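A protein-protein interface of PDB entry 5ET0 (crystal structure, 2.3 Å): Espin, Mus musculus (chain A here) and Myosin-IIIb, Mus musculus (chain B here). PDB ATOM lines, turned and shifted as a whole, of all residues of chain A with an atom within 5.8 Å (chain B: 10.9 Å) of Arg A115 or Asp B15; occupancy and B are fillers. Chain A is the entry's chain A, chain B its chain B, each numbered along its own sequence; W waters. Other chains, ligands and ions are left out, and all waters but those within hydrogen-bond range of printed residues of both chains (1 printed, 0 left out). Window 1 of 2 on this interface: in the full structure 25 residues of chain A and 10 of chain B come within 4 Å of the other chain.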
ATOM      1  N   SER A 105      29.163 -33.729  26.671  1.00  0.00           N
ATOM      2  CA  SER A 105      27.860 -34.320  26.942  1.00  0.00           C
ATOM      3  C   SER A 105      27.446 -35.360  25.906  1.00  0.00           C
ATOM      4  O   SER A 105      26.391 -35.989  26.054  1.00  0.00           O
ATOM      5  CB  SER A 105      26.806 -33.226  26.989  1.00  0.00           C
ATOM      6  OG  SER A 105      27.026 -32.425  28.138  1.00  0.00           O
ATOM      7  N   LEU A 110      24.640 -32.174  14.890  1.00  0.00           N
ATOM      8  CA  LEU A 110      23.276 -32.451  14.457  1.00  0.00           C
ATOM      9  C   LEU A 110      22.294 -32.404  15.628  1.00  0.00           C
ATOM     10  O   LEU A 110      21.143 -31.989  15.445  1.00  0.00           O
ATOM     11  CB  LEU A 110      23.208 -33.805  13.741  1.00  0.00           C
ATOM     12  CG  LEU A 110      21.809 -34.274  13.350  1.00  0.00           C
ATOM     13  CD1 LEU A 110      21.227 -33.327  12.342  1.00  0.00           C
ATOM     14  CD2 LEU A 110      21.833 -35.679  12.795  1.00  0.00           C
ATOM     15  N   HIS A 111      22.719 -32.812  16.828  1.00  0.00           N
ATOM     16  CA  HIS A 111      21.879 -32.599  18.005  1.00  0.00           C
ATOM     17  C   HIS A 111      21.556 -31.109  18.161  1.00  0.00           C
ATOM     18  O   HIS A 111      20.388 -30.709  18.161  1.00  0.00           O
ATOM     19  CB  HIS A 111      22.564 -33.140  19.266  1.00  0.00           C
ATOM     20  CG  HIS A 111      22.719 -34.634  19.300  1.00  0.00           C
ATOM     21  ND1 HIS A 111      23.815 -35.285  18.770  1.00  0.00           N
ATOM     22  CD2 HIS A 111      21.910 -35.603  19.794  1.00  0.00           C
ATOM     23  CE1 HIS A 111      23.676 -36.590  18.939  1.00  0.00           C
ATOM     24  NE2 HIS A 111      22.524 -36.808  19.549  1.00  0.00           N
ATOM     25  N   LEU A 112      22.597 -30.276  18.271  1.00  0.00           N
ATOM     26  CA  LEU A 112      22.442 -28.836  18.464  1.00  0.00           C
ATOM     27  C   LEU A 112      21.564 -28.210  17.390  1.00  0.00           C
ATOM     28  O   LEU A 112      20.663 -27.413  17.687  1.00  0.00           O
ATOM     29  CB  LEU A 112      23.820 -28.174  18.469  1.00  0.00           C
ATOM     30  CG  LEU A 112      24.821 -28.812  19.433  1.00  0.00           C
ATOM     31  CD1 LEU A 112      26.203 -28.256  19.216  1.00  0.00           C
ATOM     32  CD2 LEU A 112      24.387 -28.637  20.886  1.00  0.00           C
ATOM     33  N   ALA A 113      21.831 -28.549  16.125  1.00  0.00           N
ATOM     34  CA  ALA A 113      20.996 -28.075  15.031  1.00  0.00           C
ATOM     35  C   ALA A 113      19.531 -28.404  15.279  1.00  0.00           C
ATOM     36  O   ALA A 113      18.648 -27.588  15.007  1.00  0.00           O
ATOM     37  CB  ALA A 113      21.477 -28.693  13.710  1.00  0.00           C
ATOM     38  N   ALA A 114      19.252 -29.594  15.794  1.00  0.00           N
ATOM     39  CA  ALA A 114      17.872 -29.929  16.145  1.00  0.00           C
ATOM     40  C   ALA A 114      17.423 -29.236  17.426  1.00  0.00           C
ATOM     41  O   ALA A 114      16.248 -28.881  17.546  1.00  0.00           O
ATOM     42  CB  ALA A 114      17.705 -31.443  16.322  1.00  0.00           C
ATOM     43  N   ARG A 115      18.330 -29.056  18.390  1.00  0.00           N
ATOM     44  CA  ARG A 115      17.925 -28.548  19.694  1.00  0.00           C
ATOM     45  C   ARG A 115      17.402 -27.121  19.578  1.00  0.00           C
ATOM     46  O   ARG A 115      16.419 -26.749  20.226  1.00  0.00           O
ATOM     47  CB  ARG A 115      19.101 -28.604  20.668  1.00  0.00           C
ATOM     48  CG  ARG A 115      18.759 -28.145  22.085  1.00  0.00           C
ATOM     49  CD  ARG A 115      19.978 -28.204  22.976  1.00  0.00           C
ATOM     50  NE  ARG A 115      19.847 -27.329  24.139  1.00  0.00           N
ATOM     51  CZ  ARG A 115      20.810 -27.148  25.036  1.00  0.00           C
ATOM     52  NH1 ARG A 115      21.974 -27.799  24.911  1.00  0.00           N
ATOM     53  NH2 ARG A 115      20.617 -26.329  26.051  1.00  0.00           N
ATOM     54  N   PHE A 116      18.016 -26.329  18.710  1.00  0.00           N
ATOM     55  CA  PHE A 116      17.687 -24.928  18.560  1.00  0.00           C
ATOM     56  C   PHE A 116      16.919 -24.651  17.276  1.00  0.00           C
ATOM     57  O   PHE A 116      16.914 -23.523  16.796  1.00  0.00           O
ATOM     58  CB  PHE A 116      18.978 -24.117  18.651  1.00  0.00           C
ATOM     59  CG  PHE A 116      19.605 -24.176  20.021  1.00  0.00           C
ATOM     60  CD1 PHE A 116      18.972 -23.557  21.115  1.00  0.00           C
ATOM     61  CD2 PHE A 116      20.794 -24.852  20.232  1.00  0.00           C
ATOM     62  CE1 PHE A 116      19.520 -23.620  22.388  1.00  0.00           C
ATOM     63  CE2 PHE A 116      21.358 -24.914  21.503  1.00  0.00           C
ATOM     64  CZ  PHE A 116      20.717 -24.297  22.583  1.00  0.00           C
ATOM     65  N   GLY A 117      16.310 -25.680  16.685  1.00  0.00           N
ATOM     66  CA  GLY A 117      15.376 -25.520  15.580  1.00  0.00           C
ATOM     67  C   GLY A 117      15.833 -24.822  14.303  1.00  0.00           C
ATOM     68  O   GLY A 117      15.326 -23.753  13.958  1.00  0.00           O
ATOM     69  N   THR A 139      22.511 -38.374  27.903  1.00  0.00           N
ATOM     70  CA  THR A 139      21.183 -38.544  28.491  1.00  0.00           C
ATOM     71  C   THR A 139      20.309 -39.490  27.679  1.00  0.00           C
ATOM     72  O   THR A 139      19.226 -39.876  28.138  1.00  0.00           O
ATOM     73  CB  THR A 139      20.480 -37.197  28.623  1.00  0.00           C
ATOM     74  OG1 THR A 139      20.552 -36.534  27.361  1.00  0.00           O
ATOM     75  CG2 THR A 139      21.165 -36.330  29.660  1.00  0.00           C
ATOM     76  N   PRO A 143      18.724 -36.819  17.954  1.00  0.00           N
ATOM     77  CA  PRO A 143      18.311 -35.547  17.333  1.00  0.00           C
ATOM     78  C   PRO A 143      16.799 -35.408  17.239  1.00  0.00           C
ATOM     79  O   PRO A 143      16.274 -34.295  17.411  1.00  0.00           O
ATOM     80  CB  PRO A 143      18.980 -35.610  15.953  1.00  0.00           C
ATOM     81  CG  PRO A 143      20.183 -36.414  16.204  1.00  0.00           C
ATOM     82  CD  PRO A 143      19.802 -37.468  17.197  1.00  0.00           C
ATOM     83  N   TYR A 146      15.296 -33.847  20.258  1.00  0.00           N
ATOM     84  CA  TYR A 146      15.435 -32.395  20.335  1.00  0.00           C
ATOM     85  C   TYR A 146      14.418 -31.684  19.449  1.00  0.00           C
ATOM     86  O   TYR A 146      13.798 -30.711  19.880  1.00  0.00           O
ATOM     87  CB  TYR A 146      16.852 -31.986  19.970  1.00  0.00           C
ATOM     88  CG  TYR A 146      17.847 -32.207  21.083  1.00  0.00           C
ATOM     89  CD1 TYR A 146      17.803 -31.430  22.261  1.00  0.00           C
ATOM     90  CD2 TYR A 146      18.827 -33.191  20.974  1.00  0.00           C
ATOM     91  CE1 TYR A 146      18.725 -31.612  23.287  1.00  0.00           C
ATOM     92  CE2 TYR A 146      19.744 -33.402  22.002  1.00  0.00           C
ATOM     93  CZ  TYR A 146      19.691 -32.607  23.159  1.00  0.00           C
ATOM     94  OH  TYR A 146      20.619 -32.826  24.158  1.00  0.00           O
ATOM     95  N   ALA A 147      14.207 -32.171  18.222  1.00  0.00           N
ATOM     96  CA  ALA A 147      13.283 -31.491  17.316  1.00  0.00           C
ATOM     97  C   ALA A 147      11.858 -31.543  17.840  1.00  0.00           C
ATOM     98  O   ALA A 147      11.104 -30.566  17.719  1.00  0.00           O
ATOM     99  CB  ALA A 147      13.363 -32.105  15.920  1.00  0.00           C
ATOM    100  N   LYS A 150      11.756 -29.187  20.821  1.00  0.00           N
ATOM    101  CA  LYS A 150      11.790 -27.823  20.317  1.00  0.00           C
ATOM    102  C   LYS A 150      10.485 -27.438  19.628  1.00  0.00           C
ATOM    103  O   LYS A 150      10.158 -26.255  19.574  1.00  0.00           O
ATOM    104  CB  LYS A 150      12.979 -27.653  19.353  1.00  0.00           C
ATOM    105  CG  LYS A 150      13.124 -26.280  18.725  1.00  0.00           C
ATOM    106  CD  LYS A 150      13.131 -25.179  19.773  1.00  0.00           C
ATOM    107  CE  LYS A 150      13.078 -23.791  19.125  1.00  0.00           C
ATOM    108  NZ  LYS A 150      11.979 -23.629  18.119  1.00  0.00           N
ATOM    109  N   ILE B  11       9.627 -32.832  35.624  1.00  0.00           N
ATOM    110  CA  ILE B  11       9.626 -32.607  34.186  1.00  0.00           C
ATOM    111  C   ILE B  11      10.848 -33.298  33.585  1.00  0.00           C
ATOM    112  O   ILE B  11      11.910 -33.381  34.209  1.00  0.00           O
ATOM    113  CB  ILE B  11       9.593 -31.102  33.886  1.00  0.00           C
ATOM    114  CG1 ILE B  11      10.943 -30.475  34.213  1.00  0.00           C
ATOM    115  CG2 ILE B  11       8.512 -30.456  34.751  1.00  0.00           C
ATOM    116  CD1 ILE B  11      11.125 -29.057  33.698  1.00  0.00           C
ATOM    117  N   LYS B  12      10.699 -33.830  32.380  1.00  0.00           N
ATOM    118  CA  LYS B  12      11.786 -34.549  31.739  1.00  0.00           C
ATOM    119  C   LYS B  12      12.574 -33.581  30.876  1.00  0.00           C
ATOM    120  O   LYS B  12      12.022 -32.958  29.961  1.00  0.00           O
ATOM    121  CB  LYS B  12      11.268 -35.715  30.912  1.00  0.00           C
ATOM    122  CG  LYS B  12      10.995 -36.979  31.729  1.00  0.00           C
ATOM    123  CD  LYS B  12       9.911 -36.762  32.718  1.00  0.00           C
ATOM    124  CE  LYS B  12       9.245 -38.056  33.125  1.00  0.00           C
ATOM    125  NZ  LYS B  12       7.951 -37.720  33.863  1.00  0.00           N
ATOM    126  N   VAL B  13      13.869 -33.480  31.153  1.00  0.00           N
ATOM    127  CA  VAL B  13      14.744 -32.559  30.448  1.00  0.00           C
ATOM    128  C   VAL B  13      15.797 -33.352  29.697  1.00  0.00           C
ATOM    129  O   VAL B  13      16.131 -34.491  30.039  1.00  0.00           O
ATOM    130  CB  VAL B  13      15.417 -31.549  31.404  1.00  0.00           C
ATOM    131  CG1 VAL B  13      14.377 -30.871  32.313  1.00  0.00           C
ATOM    132  CG2 VAL B  13      16.532 -32.238  32.214  1.00  0.00           C
ATOM    133  N   LEU B  14      16.338 -32.725  28.660  1.00  0.00           N
ATOM    134  CA  LEU B  14      17.338 -33.396  27.853  1.00  0.00           C
ATOM    135  C   LEU B  14      18.753 -33.011  28.242  1.00  0.00           C
ATOM    136  O   LEU B  14      19.686 -33.797  28.006  1.00  0.00           O
ATOM    137  CB  LEU B  14      17.119 -33.079  26.368  1.00  0.00           C
ATOM    138  CG  LEU B  14      15.771 -33.510  25.799  1.00  0.00           C
ATOM    139  CD1 LEU B  14      15.616 -33.082  24.341  1.00  0.00           C
ATOM    140  CD2 LEU B  14      15.616 -35.020  25.949  1.00  0.00           C
ATOM    141  N   ASP B  15      18.927 -31.842  28.855  1.00  0.00           N
ATOM    142  CA  ASP B  15      20.239 -31.318  29.203  1.00  0.00           C
ATOM    143  C   ASP B  15      20.263 -30.840  30.649  1.00  0.00           C
ATOM    144  O   ASP B  15      19.237 -30.759  31.331  1.00  0.00           O
ATOM    145  CB  ASP B  15      20.638 -30.172  28.257  1.00  0.00           C
ATOM    146  CG  ASP B  15      21.062 -30.681  26.875  1.00  0.00           C
ATOM    147  OD1 ASP B  15      22.267 -30.987  26.708  1.00  0.00           O
ATOM    148  OD2 ASP B  15      20.187 -30.784  25.975  1.00  0.00           O
ATOM    149  N   GLY B  16      21.475 -30.542  31.110  1.00  0.00           N
ATOM    150  CA  GLY B  16      21.686 -29.984  32.424  1.00  0.00           C
ATOM    151  C   GLY B  16      21.405 -28.493  32.394  1.00  0.00           C
ATOM    152  O   GLY B  16      20.964 -27.927  31.391  1.00  0.00           O
ATOM    153  N   GLU B  17      21.684 -27.843  33.520  1.00  0.00           N
ATOM    154  CA  GLU B  17      21.432 -26.417  33.632  1.00  0.00           C
ATOM    155  C   GLU B  17      22.584 -25.569  33.070  1.00  0.00           C
ATOM    156  O   GLU B  17      22.572 -24.341  33.253  1.00  0.00           O
ATOM    157  CB  GLU B  17      21.152 -26.037  35.095  1.00  0.00           C
ATOM    158  N   ASP B  18      23.584 -26.191  32.436  1.00  0.00           N
ATOM    159  CA  ASP B  18      24.679 -25.436  31.840  1.00  0.00           C
ATOM    160  C   ASP B  18      24.110 -24.447  30.826  1.00  0.00           C
ATOM    161  O   ASP B  18      23.181 -24.759  30.080  1.00  0.00           O
ATOM    162  CB  ASP B  18      25.682 -26.386  31.175  1.00  0.00           C
ATOM    163  CG  ASP B  18      26.781 -25.654  30.400  1.00  0.00           C
ATOM    164  OD1 ASP B  18      26.913 -24.424  30.561  1.00  0.00           O
ATOM    165  OD2 ASP B  18      27.514 -26.316  29.625  1.00  0.00           O
ATOM    166  N   GLN B  19      24.655 -23.238  30.818  1.00  0.00           N
ATOM    167  CA  GLN B  19      24.118 -22.162  30.000  1.00  0.00           C
ATOM    168  C   GLN B  19      24.942 -21.861  28.748  1.00  0.00           C
ATOM    169  O   GLN B  19      24.602 -20.928  28.020  1.00  0.00           O
ATOM    170  CB  GLN B  19      23.969 -20.898  30.865  1.00  0.00           C
ATOM    171  N   TYR B  20      25.960 -22.665  28.430  1.00  0.00           N
ATOM    172  CA  TYR B  20      26.841 -22.320  27.315  1.00  0.00           C
ATOM    173  C   TYR B  20      26.090 -22.164  25.993  1.00  0.00           C
ATOM    174  O   TYR B  20      26.276 -21.164  25.293  1.00  0.00           O
ATOM    175  CB  TYR B  20      27.991 -23.331  27.221  1.00  0.00           C
ATOM    176  CG  TYR B  20      28.925 -23.107  26.045  1.00  0.00           C
ATOM    177  CD1 TYR B  20      28.514 -23.359  24.732  1.00  0.00           C
ATOM    178  CD2 TYR B  20      30.166 -22.518  26.236  1.00  0.00           C
ATOM    179  CE1 TYR B  20      29.345 -23.116  23.662  1.00  0.00           C
ATOM    180  CE2 TYR B  20      30.996 -22.262  25.173  1.00  0.00           C
ATOM    181  CZ  TYR B  20      30.582 -22.566  23.887  1.00  0.00           C
ATOM    182  OH  TYR B  20      31.409 -22.309  22.836  1.00  0.00           O
ATOM    183  N   TYR B  21      25.233 -23.116  25.630  1.00  0.00           N
ATOM    184  CA  TYR B  21      24.557 -22.958  24.343  1.00  0.00           C
ATOM    185  C   TYR B  21      23.407 -21.968  24.390  1.00  0.00           C
ATOM    186  O   TYR B  21      23.211 -21.221  23.425  1.00  0.00           O
ATOM    187  CB  TYR B  21      24.065 -24.290  23.784  1.00  0.00           C
ATOM    188  CG  TYR B  21      25.173 -25.251  23.490  1.00  0.00           C
ATOM    189  CD1 TYR B  21      25.822 -25.228  22.258  1.00  0.00           C
ATOM    190  CD2 TYR B  21      25.531 -26.226  24.406  1.00  0.00           C
ATOM    191  CE1 TYR B  21      26.820 -26.117  21.974  1.00  0.00           C
ATOM    192  CE2 TYR B  21      26.531 -27.122  24.128  1.00  0.00           C
ATOM    193  CZ  TYR B  21      27.170 -27.078  22.910  1.00  0.00           C
ATOM    194  OH  TYR B  21      28.172 -27.999  22.652  1.00  0.00           O
ATOM    195  N   LYS B  22      22.616 -21.957  25.470  1.00  0.00           N
ATOM    196  CA  LYS B  22      21.517 -21.003  25.516  1.00  0.00           C
ATOM    197  C   LYS B  22      22.067 -19.594  25.436  1.00  0.00           C
ATOM    198  O   LYS B  22      21.587 -18.770  24.649  1.00  0.00           O
ATOM    199  CB  LYS B  22      20.695 -21.179  26.797  1.00  0.00           C
ATOM    200  N   CYS B  23      23.148 -19.336  26.164  1.00  0.00           N
ATOM    201  CA  CYS B  23      23.780 -18.022  26.186  1.00  0.00           C
ATOM    202  C   CYS B  23      24.806 -17.911  25.061  1.00  0.00           C
ATOM    203  O   CYS B  23      25.977 -17.607  25.281  1.00  0.00           O
ATOM    204  CB  CYS B  23      24.421 -17.794  27.544  1.00  0.00           C
ATOM    205  SG  CYS B  23      23.202 -17.943  28.869  1.00  0.00           S
ATOM    206  N   LEU B  24      24.318 -18.121  23.833  1.00  0.00           N
ATOM    207  CA  LEU B  24      25.107 -17.967  22.617  1.00  0.00           C
ATOM    208  C   LEU B  24      24.446 -16.990  21.665  1.00  0.00           C
ATOM    209  O   LEU B  24      25.138 -16.267  20.949  1.00  0.00           O
ATOM    210  CB  LEU B  24      25.310 -19.315  21.900  1.00  0.00           C
ATOM    211  CG  LEU B  24      26.552 -20.124  22.311  1.00  0.00           C
ATOM    212  CD1 LEU B  24      26.627 -21.450  21.588  1.00  0.00           C
ATOM    213  CD2 LEU B  24      27.830 -19.358  22.155  1.00  0.00           C
ATOM    214  N   SER B  25      23.126 -16.967  21.643  1.00  0.00           N
ATOM    215  CA  SER B  25      22.362 -15.967  20.938  1.00  0.00           C
ATOM    216  C   SER B  25      22.300 -14.789  21.910  1.00  0.00           C
ATOM    217  O   SER B  25      22.735 -14.916  23.058  1.00  0.00           O
ATOM    218  CB  SER B  25      21.012 -16.572  20.547  1.00  0.00           C
ATOM    219  OG  SER B  25      19.957 -15.636  20.471  1.00  0.00           O
HETATM  220  O   HOH W   1      21.375 -34.605  25.907  1.00  0.00           O
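The side-chain carboxylate of Asp B15 lies within salt-bridge range of the guanidinium group of Arg A115, 3.6 Å away.
The side-chain hydroxyl (OG1) of Thr A139 lies within hydrogen-bond range of the backbone carbonyl oxygen (O) of Leu B14, at 2.9 Å.
OH of Tyr A146 is in hydrogen-bond range of OD2 of Asp B15 (2.8 Å).
Leu A112 touches Tyr B21.
NH1 of Arg A115 touches CD2 of Tyr B21, at 3.9 Å.
Phe A116 touches Tyr B21.
CD1 of Leu B14 touches CD1 of Tyr A146, at 3.4 Å.
Of the printed residues of chain B, Leu A112 touches Tyr B21.
No residue of chain B comes within 4 Å of Ala A113.
Of the printed residues of chain B, Arg A115 touches Asp B15 (3.6 Å) and Tyr B21 (3.9 Å).
Phe A116 touches just one residue of chain B: Tyr B21 (3.6 Å).
Of the printed residues of chain B, Thr A139 touches Leu B14 (2.9 Å).
No residue of chain B comes within 4 Å of Lys A150.
Of the printed residues of chain A, Leu B14 touches Thr A139 (2.9 Å) and Tyr A146 (3.4 Å).
Of chain A, only Arg A115 and Tyr A146 come within 4 Å of Asp B15.
Printed residues of chain A within 4 Å of Tyr B21: Leu A112 (3.5 Å), Arg A115 (3.9 Å) and Phe A116 (3.6 Å).
Printed residues of chain A that touch a printed residue of chain B: Leu A112, Arg A115, Phe A116, Thr A139 and Tyr A146.
Hydrophobic or aromatic side chains of chain A within 4 Å of the printed part of chain B: Leu A112, Phe A116 and Tyr A146.
Of the 15 printed residues of chain B, 3 touch a printed residue of chain A.
Among the printed residues, 7 pairs touch across the chains.
Among the printed residues, Asp or Glu carboxylates within 4 Å of a Lys or Arg side-chain nitrogen of the other chain: Arg A115 with Asp B15.
Water W1 lies within hydrogen-bond range of the side-chain hydroxyl of Thr A139 (2.6 Å), the side-chain hydroxyl of Tyr A146 (2.6 Å) and the backbone carbonyl oxygen of Leu B14 (2.8 Å).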
